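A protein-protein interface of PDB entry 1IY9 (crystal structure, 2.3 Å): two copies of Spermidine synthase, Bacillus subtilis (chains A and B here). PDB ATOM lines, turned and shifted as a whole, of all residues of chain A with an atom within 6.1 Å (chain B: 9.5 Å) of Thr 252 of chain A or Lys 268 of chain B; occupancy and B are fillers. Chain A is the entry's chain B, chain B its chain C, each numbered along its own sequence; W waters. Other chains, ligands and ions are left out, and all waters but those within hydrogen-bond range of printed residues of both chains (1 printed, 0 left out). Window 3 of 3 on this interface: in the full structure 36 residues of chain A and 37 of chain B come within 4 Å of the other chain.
Water W1 bridges the backbone carbonyl oxygen of Leu 266 of chain B and the side-chain hydroxyl of Thr 256 of chain A.
Thr 252 of chain A touches just one residue of chain B: Lys 268. Of the printed residues of chain A, Lys 268 of chain B touches Thr 252 (3.5 Å), Lys 253 (3.6 Å), Tyr 254 (2.9 Å) and Thr 256 (3.95 Å). Printed residues of chain A within 4 Å of Pro 267 of chain B: Tyr 254 (3.5 Å) and Ile 259 (3.9 Å). Of the printed residues of chain B, Tyr 254 of chain A touches Pro 267 (3.5 Å) and Lys 268 (2.9 Å). Of the printed residues of chain A, Val 265 of chain B touches Ile 259 (3.7 Å). Of the printed residues of chain B, Thr 256 of chain A touches Lys 268 (3.95 Å). Printed residues of chain B within 4 Å of Lys 253 of chain A: Lys 268 (3.6 Å) and Phe 269 (2.8 Å). His 67 of chain A touches none of the printed residues of chain B. Ser 271 of chain B touches none of the printed residues of chain A. The nearest residue of chain A that does not touch Lys 268 of chain B is Tyr 255 of chain A (4.1 Å).
Among the printed residues, pairs that only touch across the chains: Thr 252 of chain A with Lys 268 of chain B, Lys 253 of chain A with Lys 268 of chain B, Tyr 254 of chain A with Pro 267 of chain B, Thr 256 of chain A with Lys 268 of chain B, Ile 259 of chain A with Val 265 of chain B, Ile 259 of chain A with Leu 266 of chain B and Ile 259 of chain A with Pro 267 of chain B.
No position is printed for both chains.
Of the 13 printed residues of chain B, 5 touch a printed residue of chain A. Of the 12 printed residues of chain A, 5 touch a printed residue of chain B. Hydrophobic or aromatic side chains of chain A that line the printed part of chain B: Tyr 254 and Ile 259. Among the printed residues, 9 pairs touch across the chains. Among the printed residues, no Asp or Glu carboxylate lies within 4 Å of a Lys or Arg side-chain nitrogen of the other chain.
The backbone NH (N) of Lys 268 of chain B sits at hydrogen-bond distance from the backbone carbonyl oxygen (O) of Tyr 254 of chain A (2.9 Å). O of Lys 253 of chain A sits at hydrogen-bond distance from N of Phe 269 of chain B (2.8 Å).
The backbone NH (N) of Tyr 254 of chain A sits at hydrogen-bond distance from the side-chain carboxylate (OE1) of Glu 63 of chain A (2.9 Å). The side-chain hydroxyl of Ser 271 of chain B lies within hydrogen-bond range of the backbone carbonyl oxygen of Pro 267 of chain B (3.3 Å). NZ of Lys 268 of chain B lies within salt-bridge range of OD1 of Asp 272 of chain B. OG1 of Thr 252 of chain A is in hydrogen-bond range of O of Tyr 255 of chain A (2.7 Å). N of Lys 253 of chain A lies within hydrogen-bond range of OE2 of Glu 63 of chain A, 2.8 Å away.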
ATOM      1  N   GLU A  63       8.723 -21.535 -19.160  1.00  0.00           N
ATOM      2  CA  GLU A  63       7.861 -22.600 -18.672  1.00  0.00           C
ATOM      3  C   GLU A  63       6.902 -22.198 -17.568  1.00  0.00           C
ATOM      4  O   GLU A  63       5.764 -22.602 -17.573  1.00  0.00           O
ATOM      5  CB  GLU A  63       8.701 -23.758 -18.181  1.00  0.00           C
ATOM      6  CG  GLU A  63       9.370 -24.512 -19.263  1.00  0.00           C
ATOM      7  CD  GLU A  63      10.289 -25.552 -18.702  1.00  0.00           C
ATOM      8  OE1 GLU A  63      10.234 -25.769 -17.484  1.00  0.00           O
ATOM      9  OE2 GLU A  63      11.067 -26.151 -19.462  1.00  0.00           O
ATOM     10  N   HIS A  67       3.004 -22.673 -18.480  1.00  0.00           N
ATOM     11  CA  HIS A  67       2.353 -23.831 -17.907  1.00  0.00           C
ATOM     12  C   HIS A  67       1.504 -23.702 -16.649  1.00  0.00           C
ATOM     13  O   HIS A  67       0.594 -24.511 -16.443  1.00  0.00           O
ATOM     14  CB  HIS A  67       3.359 -24.954 -17.735  1.00  0.00           C
ATOM     15  CG  HIS A  67       4.096 -25.295 -18.991  1.00  0.00           C
ATOM     16  ND1 HIS A  67       3.459 -25.486 -20.197  1.00  0.00           N
ATOM     17  CD2 HIS A  67       5.416 -25.461 -19.233  1.00  0.00           C
ATOM     18  CE1 HIS A  67       4.352 -25.759 -21.129  1.00  0.00           C
ATOM     19  NE2 HIS A  67       5.546 -25.747 -20.569  1.00  0.00           N
ATOM     20  N   GLU A  92       6.353 -22.740 -25.569  1.00  0.00           N
ATOM     21  CA  GLU A  92       5.778 -23.534 -24.478  1.00  0.00           C
ATOM     22  C   GLU A  92       4.267 -23.718 -24.599  1.00  0.00           C
ATOM     23  O   GLU A  92       3.735 -24.774 -24.225  1.00  0.00           O
ATOM     24  CB  GLU A  92       6.136 -22.924 -23.118  1.00  0.00           C
ATOM     25  CG  GLU A  92       7.645 -22.925 -22.814  1.00  0.00           C
ATOM     26  CD  GLU A  92       8.259 -24.315 -22.792  1.00  0.00           C
ATOM     27  OE1 GLU A  92       9.443 -24.451 -23.166  1.00  0.00           O
ATOM     28  OE2 GLU A  92       7.568 -25.286 -22.400  1.00  0.00           O
ATOM     29  N   LYS A  95       3.008 -26.624 -26.691  1.00  0.00           N
ATOM     30  CA  LYS A  95       3.100 -27.979 -26.167  1.00  0.00           C
ATOM     31  C   LYS A  95       1.721 -28.464 -25.681  1.00  0.00           C
ATOM     32  O   LYS A  95       1.552 -29.636 -25.317  1.00  0.00           O
ATOM     33  CB  LYS A  95       4.117 -28.048 -25.040  1.00  0.00           C
ATOM     34  CG  LYS A  95       5.539 -27.761 -25.501  1.00  0.00           C
ATOM     35  CD  LYS A  95       6.546 -27.839 -24.359  1.00  0.00           C
ATOM     36  CE  LYS A  95       7.933 -27.461 -24.844  1.00  0.00           C
ATOM     37  NZ  LYS A  95       8.959 -27.373 -23.772  1.00  0.00           N
ATOM     38  N   ILE A 250       4.595 -33.726 -20.826  1.00  0.00           N
ATOM     39  CA  ILE A 250       5.017 -32.555 -21.557  1.00  0.00           C
ATOM     40  C   ILE A 250       6.502 -32.440 -21.267  1.00  0.00           C
ATOM     41  O   ILE A 250       6.960 -32.764 -20.156  1.00  0.00           O
ATOM     42  CB  ILE A 250       4.228 -31.329 -21.042  1.00  0.00           C
ATOM     43  CG1 ILE A 250       4.296 -30.180 -22.016  1.00  0.00           C
ATOM     44  CG2 ILE A 250       4.721 -30.889 -19.676  1.00  0.00           C
ATOM     45  CD1 ILE A 250       3.333 -29.102 -21.645  1.00  0.00           C
ATOM     46  N   GLU A 251       7.270 -32.067 -22.281  1.00  0.00           N
ATOM     47  CA  GLU A 251       8.703 -31.951 -22.109  1.00  0.00           C
ATOM     48  C   GLU A 251       9.093 -30.603 -21.545  1.00  0.00           C
ATOM     49  O   GLU A 251       8.826 -29.570 -22.158  1.00  0.00           O
ATOM     50  CB  GLU A 251       9.393 -32.169 -23.422  1.00  0.00           C
ATOM     51  CG  GLU A 251      10.804 -32.586 -23.229  1.00  0.00           C
ATOM     52  CD  GLU A 251      11.516 -32.792 -24.541  1.00  0.00           C
ATOM     53  OE1 GLU A 251      12.763 -32.944 -24.525  1.00  0.00           O
ATOM     54  OE2 GLU A 251      10.831 -32.799 -25.592  1.00  0.00           O
ATOM     55  N   THR A 252       9.671 -30.618 -20.348  1.00  0.00           N
ATOM     56  CA  THR A 252      10.101 -29.402 -19.664  1.00  0.00           C
ATOM     57  C   THR A 252      11.396 -29.677 -18.901  1.00  0.00           C
ATOM     58  O   THR A 252      11.777 -30.837 -18.699  1.00  0.00           O
ATOM     59  CB  THR A 252       9.052 -28.882 -18.653  1.00  0.00           C
ATOM     60  OG1 THR A 252       8.808 -29.885 -17.670  1.00  0.00           O
ATOM     61  CG2 THR A 252       7.744 -28.488 -19.335  1.00  0.00           C
ATOM     62  N   LYS A 253      12.079 -28.609 -18.497  1.00  0.00           N
ATOM     63  CA  LYS A 253      13.340 -28.731 -17.766  1.00  0.00           C
ATOM     64  C   LYS A 253      13.241 -28.134 -16.359  1.00  0.00           C
ATOM     65  O   LYS A 253      14.167 -28.269 -15.558  1.00  0.00           O
ATOM     66  CB  LYS A 253      14.481 -28.038 -18.516  1.00  0.00           C
ATOM     67  CG  LYS A 253      14.734 -28.537 -19.920  1.00  0.00           C
ATOM     68  CD  LYS A 253      15.853 -27.745 -20.528  1.00  0.00           C
ATOM     69  CE  LYS A 253      15.647 -27.489 -22.009  1.00  0.00           C
ATOM     70  NZ  LYS A 253      16.670 -26.520 -22.491  1.00  0.00           N
ATOM     71  N   TYR A 254      12.116 -27.499 -16.057  1.00  0.00           N
ATOM     72  CA  TYR A 254      11.919 -26.894 -14.764  1.00  0.00           C
ATOM     73  C   TYR A 254      10.548 -27.282 -14.225  1.00  0.00           C
ATOM     74  O   TYR A 254      10.439 -27.942 -13.195  1.00  0.00           O
ATOM     75  CB  TYR A 254      12.020 -25.370 -14.874  1.00  0.00           C
ATOM     76  CG  TYR A 254      12.019 -24.656 -13.541  1.00  0.00           C
ATOM     77  CD1 TYR A 254      13.211 -24.277 -12.930  1.00  0.00           C
ATOM     78  CD2 TYR A 254      10.822 -24.378 -12.879  1.00  0.00           C
ATOM     79  CE1 TYR A 254      13.207 -23.637 -11.692  1.00  0.00           C
ATOM     80  CE2 TYR A 254      10.809 -23.747 -11.641  1.00  0.00           C
ATOM     81  CZ  TYR A 254      12.000 -23.371 -11.050  1.00  0.00           C
ATOM     82  OH  TYR A 254      11.979 -22.690  -9.838  1.00  0.00           O
ATOM     83  N   TYR A 255       9.510 -26.830 -14.911  1.00  0.00           N
ATOM     84  CA  TYR A 255       8.131 -27.087 -14.535  1.00  0.00           C
ATOM     85  C   TYR A 255       7.819 -28.557 -14.338  1.00  0.00           C
ATOM     86  O   TYR A 255       8.267 -29.403 -15.094  1.00  0.00           O
ATOM     87  CB  TYR A 255       7.176 -26.479 -15.555  1.00  0.00           C
ATOM     88  CG  TYR A 255       5.735 -26.694 -15.204  1.00  0.00           C
ATOM     89  CD1 TYR A 255       5.052 -25.776 -14.416  1.00  0.00           C
ATOM     90  CD2 TYR A 255       5.044 -27.830 -15.649  1.00  0.00           C
ATOM     91  CE1 TYR A 255       3.732 -25.974 -14.076  1.00  0.00           C
ATOM     92  CE2 TYR A 255       3.708 -28.042 -15.312  1.00  0.00           C
ATOM     93  CZ  TYR A 255       3.062 -27.110 -14.523  1.00  0.00           C
ATOM     94  OH  TYR A 255       1.757 -27.298 -14.158  1.00  0.00           O
ATOM     95  N   THR A 256       6.965 -28.811 -13.358  1.00  0.00           N
ATOM     96  CA  THR A 256       6.547 -30.139 -12.940  1.00  0.00           C
ATOM     97  C   THR A 256       5.176 -29.935 -12.340  1.00  0.00           C
ATOM     98  O   THR A 256       4.877 -28.839 -11.891  1.00  0.00           O
ATOM     99  CB  THR A 256       7.496 -30.630 -11.825  1.00  0.00           C
ATOM    100  OG1 THR A 256       8.657 -31.235 -12.406  1.00  0.00           O
ATOM    101  CG2 THR A 256       6.821 -31.605 -10.921  1.00  0.00           C
ATOM    102  N   ILE A 259       5.869 -28.864  -8.958  1.00  0.00           N
ATOM    103  CA  ILE A 259       6.411 -27.505  -8.927  1.00  0.00           C
ATOM    104  C   ILE A 259       5.232 -26.545  -9.101  1.00  0.00           C
ATOM    105  O   ILE A 259       5.189 -25.461  -8.507  1.00  0.00           O
ATOM    106  CB  ILE A 259       7.452 -27.265 -10.058  1.00  0.00           C
ATOM    107  CG1 ILE A 259       8.840 -27.621  -9.557  1.00  0.00           C
ATOM    108  CG2 ILE A 259       7.455 -25.807 -10.508  1.00  0.00           C
ATOM    109  CD1 ILE A 259       9.232 -26.825  -8.290  1.00  0.00           C
ATOM    110  N   PRO B 192      22.706 -26.088  -8.375  1.00  0.00           N
ATOM    111  CA  PRO B 192      22.576 -27.025  -9.495  1.00  0.00           C
ATOM    112  C   PRO B 192      22.938 -26.472 -10.864  1.00  0.00           C
ATOM    113  O   PRO B 192      22.892 -27.197 -11.840  1.00  0.00           O
ATOM    114  CB  PRO B 192      21.097 -27.390  -9.431  1.00  0.00           C
ATOM    115  CG  PRO B 192      20.483 -26.080  -9.063  1.00  0.00           C
ATOM    116  CD  PRO B 192      21.386 -25.568  -7.971  1.00  0.00           C
ATOM    117  N   LEU B 227      20.003 -20.056  -6.155  1.00  0.00           N
ATOM    118  CA  LEU B 227      19.350 -21.263  -5.684  1.00  0.00           C
ATOM    119  C   LEU B 227      20.408 -22.114  -5.024  1.00  0.00           C
ATOM    120  O   LEU B 227      21.377 -22.519  -5.673  1.00  0.00           O
ATOM    121  CB  LEU B 227      18.738 -22.042  -6.852  1.00  0.00           C
ATOM    122  CG  LEU B 227      17.990 -23.321  -6.456  1.00  0.00           C
ATOM    123  CD1 LEU B 227      16.828 -22.939  -5.556  1.00  0.00           C
ATOM    124  CD2 LEU B 227      17.508 -24.082  -7.707  1.00  0.00           C
ATOM    125  N   PHE B 264      11.452 -29.350  -0.684  1.00  0.00           N
ATOM    126  CA  PHE B 264      11.865 -30.657  -1.218  1.00  0.00           C
ATOM    127  C   PHE B 264      11.296 -30.945  -2.610  1.00  0.00           C
ATOM    128  O   PHE B 264      11.543 -32.009  -3.166  1.00  0.00           O
ATOM    129  CB  PHE B 264      11.456 -31.783  -0.259  1.00  0.00           C
ATOM    130  CG  PHE B 264      12.223 -31.792   1.048  1.00  0.00           C
ATOM    131  CD1 PHE B 264      11.832 -30.971   2.110  1.00  0.00           C
ATOM    132  CD2 PHE B 264      13.371 -32.569   1.190  1.00  0.00           C
ATOM    133  CE1 PHE B 264      12.576 -30.917   3.280  1.00  0.00           C
ATOM    134  CE2 PHE B 264      14.118 -32.513   2.365  1.00  0.00           C
ATOM    135  CZ  PHE B 264      13.717 -31.680   3.409  1.00  0.00           C
ATOM    136  N   VAL B 265      10.456 -30.052  -3.131  1.00  0.00           N
ATOM    137  CA  VAL B 265       9.878 -30.223  -4.471  1.00  0.00           C
ATOM    138  C   VAL B 265      10.891 -29.570  -5.411  1.00  0.00           C
ATOM    139  O   VAL B 265      11.021 -28.339  -5.482  1.00  0.00           O
ATOM    140  CB  VAL B 265       8.512 -29.524  -4.604  1.00  0.00           C
ATOM    141  CG1 VAL B 265       7.919 -29.778  -5.960  1.00  0.00           C
ATOM    142  CG2 VAL B 265       7.565 -30.004  -3.532  1.00  0.00           C
ATOM    143  N   LEU B 266      11.633 -30.414  -6.102  1.00  0.00           N
ATOM    144  CA  LEU B 266      12.670 -29.974  -6.983  1.00  0.00           C
ATOM    145  C   LEU B 266      12.270 -29.716  -8.428  1.00  0.00           C
ATOM    146  O   LEU B 266      11.395 -30.382  -8.960  1.00  0.00           O
ATOM    147  CB  LEU B 266      13.779 -31.024  -6.963  1.00  0.00           C
ATOM    148  CG  LEU B 266      14.794 -31.161  -5.823  1.00  0.00           C
ATOM    149  CD1 LEU B 266      14.506 -30.242  -4.658  1.00  0.00           C
ATOM    150  CD2 LEU B 266      14.850 -32.586  -5.413  1.00  0.00           C
ATOM    151  N   PRO B 267      12.869 -28.688  -9.061  1.00  0.00           N
ATOM    152  CA  PRO B 267      12.573 -28.380 -10.461  1.00  0.00           C
ATOM    153  C   PRO B 267      13.082 -29.608 -11.230  1.00  0.00           C
ATOM    154  O   PRO B 267      14.077 -30.236 -10.855  1.00  0.00           O
ATOM    155  CB  PRO B 267      13.483 -27.185 -10.738  1.00  0.00           C
ATOM    156  CG  PRO B 267      13.518 -26.489  -9.429  1.00  0.00           C
ATOM    157  CD  PRO B 267      13.690 -27.621  -8.456  1.00  0.00           C
ATOM    158  N   LYS B 268      12.408 -29.938 -12.309  1.00  0.00           N
ATOM    159  CA  LYS B 268      12.779 -31.076 -13.125  1.00  0.00           C
ATOM    160  C   LYS B 268      14.266 -31.296 -13.337  1.00  0.00           C
ATOM    161  O   LYS B 268      14.766 -32.378 -13.059  1.00  0.00           O
ATOM    162  CB  LYS B 268      12.033 -31.001 -14.451  1.00  0.00           C
ATOM    163  CG  LYS B 268      12.481 -31.960 -15.501  1.00  0.00           C
ATOM    164  CD  LYS B 268      12.212 -33.386 -15.154  1.00  0.00           C
ATOM    165  CE  LYS B 268      12.699 -34.219 -16.335  1.00  0.00           C
ATOM    166  NZ  LYS B 268      12.506 -35.683 -16.141  1.00  0.00           N
ATOM    167  N   PHE B 269      15.002 -30.276 -13.755  1.00  0.00           N
ATOM    168  CA  PHE B 269      16.430 -30.463 -13.996  1.00  0.00           C
ATOM    169  C   PHE B 269      17.266 -30.791 -12.752  1.00  0.00           C
ATOM    170  O   PHE B 269      18.374 -31.347 -12.857  1.00  0.00           O
ATOM    171  CB  PHE B 269      17.018 -29.280 -14.787  1.00  0.00           C
ATOM    172  CG  PHE B 269      17.400 -28.079 -13.938  1.00  0.00           C
ATOM    173  CD1 PHE B 269      18.729 -27.845 -13.596  1.00  0.00           C
ATOM    174  CD2 PHE B 269      16.438 -27.190 -13.490  1.00  0.00           C
ATOM    175  CE1 PHE B 269      19.090 -26.743 -12.821  1.00  0.00           C
ATOM    176  CE2 PHE B 269      16.788 -26.080 -12.711  1.00  0.00           C
ATOM    177  CZ  PHE B 269      18.114 -25.858 -12.376  1.00  0.00           C
ATOM    178  N   VAL B 270      16.756 -30.414 -11.578  1.00  0.00           N
ATOM    179  CA  VAL B 270      17.453 -30.673 -10.317  1.00  0.00           C
ATOM    180  C   VAL B 270      17.220 -32.117  -9.870  1.00  0.00           C
ATOM    181  O   VAL B 270      18.152 -32.740  -9.349  1.00  0.00           O
ATOM    182  CB  VAL B 270      17.057 -29.667  -9.187  1.00  0.00           C
ATOM    183  CG1 VAL B 270      17.829 -29.971  -7.922  1.00  0.00           C
ATOM    184  CG2 VAL B 270      17.374 -28.258  -9.614  1.00  0.00           C
ATOM    185  N   SER B 271      15.995 -32.637 -10.065  1.00  0.00           N
ATOM    186  CA  SER B 271      15.685 -34.026  -9.744  1.00  0.00           C
ATOM    187  C   SER B 271      16.603 -34.896 -10.590  1.00  0.00           C
ATOM    188  O   SER B 271      17.162 -35.887 -10.101  1.00  0.00           O
ATOM    189  CB  SER B 271      14.270 -34.386 -10.152  1.00  0.00           C
ATOM    190  OG  SER B 271      13.380 -33.344  -9.882  1.00  0.00           O
ATOM    191  N   ASP B 272      16.757 -34.530 -11.864  1.00  0.00           N
ATOM    192  CA  ASP B 272      17.622 -35.281 -12.785  1.00  0.00           C
ATOM    193  C   ASP B 272      19.048 -35.505 -12.274  1.00  0.00           C
ATOM    194  O   ASP B 272      19.737 -36.394 -12.732  1.00  0.00           O
ATOM    195  CB  ASP B 272      17.700 -34.588 -14.142  1.00  0.00           C
ATOM    196  CG  ASP B 272      16.402 -34.674 -14.936  1.00  0.00           C
ATOM    197  OD1 ASP B 272      15.402 -35.265 -14.451  1.00  0.00           O
ATOM    198  OD2 ASP B 272      16.390 -34.145 -16.073  1.00  0.00           O
ATOM    199  N   LEU B 273      19.516 -34.640 -11.385  1.00  0.00           N
ATOM    200  CA  LEU B 273      20.858 -34.755 -10.833  1.00  0.00           C
ATOM    201  C   LEU B 273      20.995 -35.887  -9.824  1.00  0.00           C
ATOM    202  O   LEU B 273      22.089 -36.397  -9.626  1.00  0.00           O
ATOM    203  CB  LEU B 273      21.291 -33.430 -10.189  1.00  0.00           C
ATOM    204  CG  LEU B 273      21.521 -32.248 -11.138  1.00  0.00           C
ATOM    205  CD1 LEU B 273      21.953 -31.018 -10.364  1.00  0.00           C
ATOM    206  CD2 LEU B 273      22.575 -32.577 -12.132  1.00  0.00           C
ATOM    207  N   ILE B 274      19.911 -36.225  -9.133  1.00  0.00           N
ATOM    208  CA  ILE B 274      19.956 -37.301  -8.159  1.00  0.00           C
ATOM    209  C   ILE B 274      19.393 -38.585  -8.774  1.00  0.00           C
ATOM    210  O   ILE B 274      18.220 -38.608  -9.221  1.00  0.00           O
ATOM    211  CB  ILE B 274      19.293 -36.936  -6.771  1.00  0.00           C
ATOM    212  CG1 ILE B 274      18.465 -38.111  -6.240  1.00  0.00           C
ATOM    213  CG2 ILE B 274      18.511 -35.627  -6.810  1.00  0.00           C
ATOM    214  CD1 ILE B 274      17.809 -37.884  -4.839  1.00  0.00           C
HETATM  215  O   HOH W   1       8.817 -30.912  -9.026  1.00  0.00           O
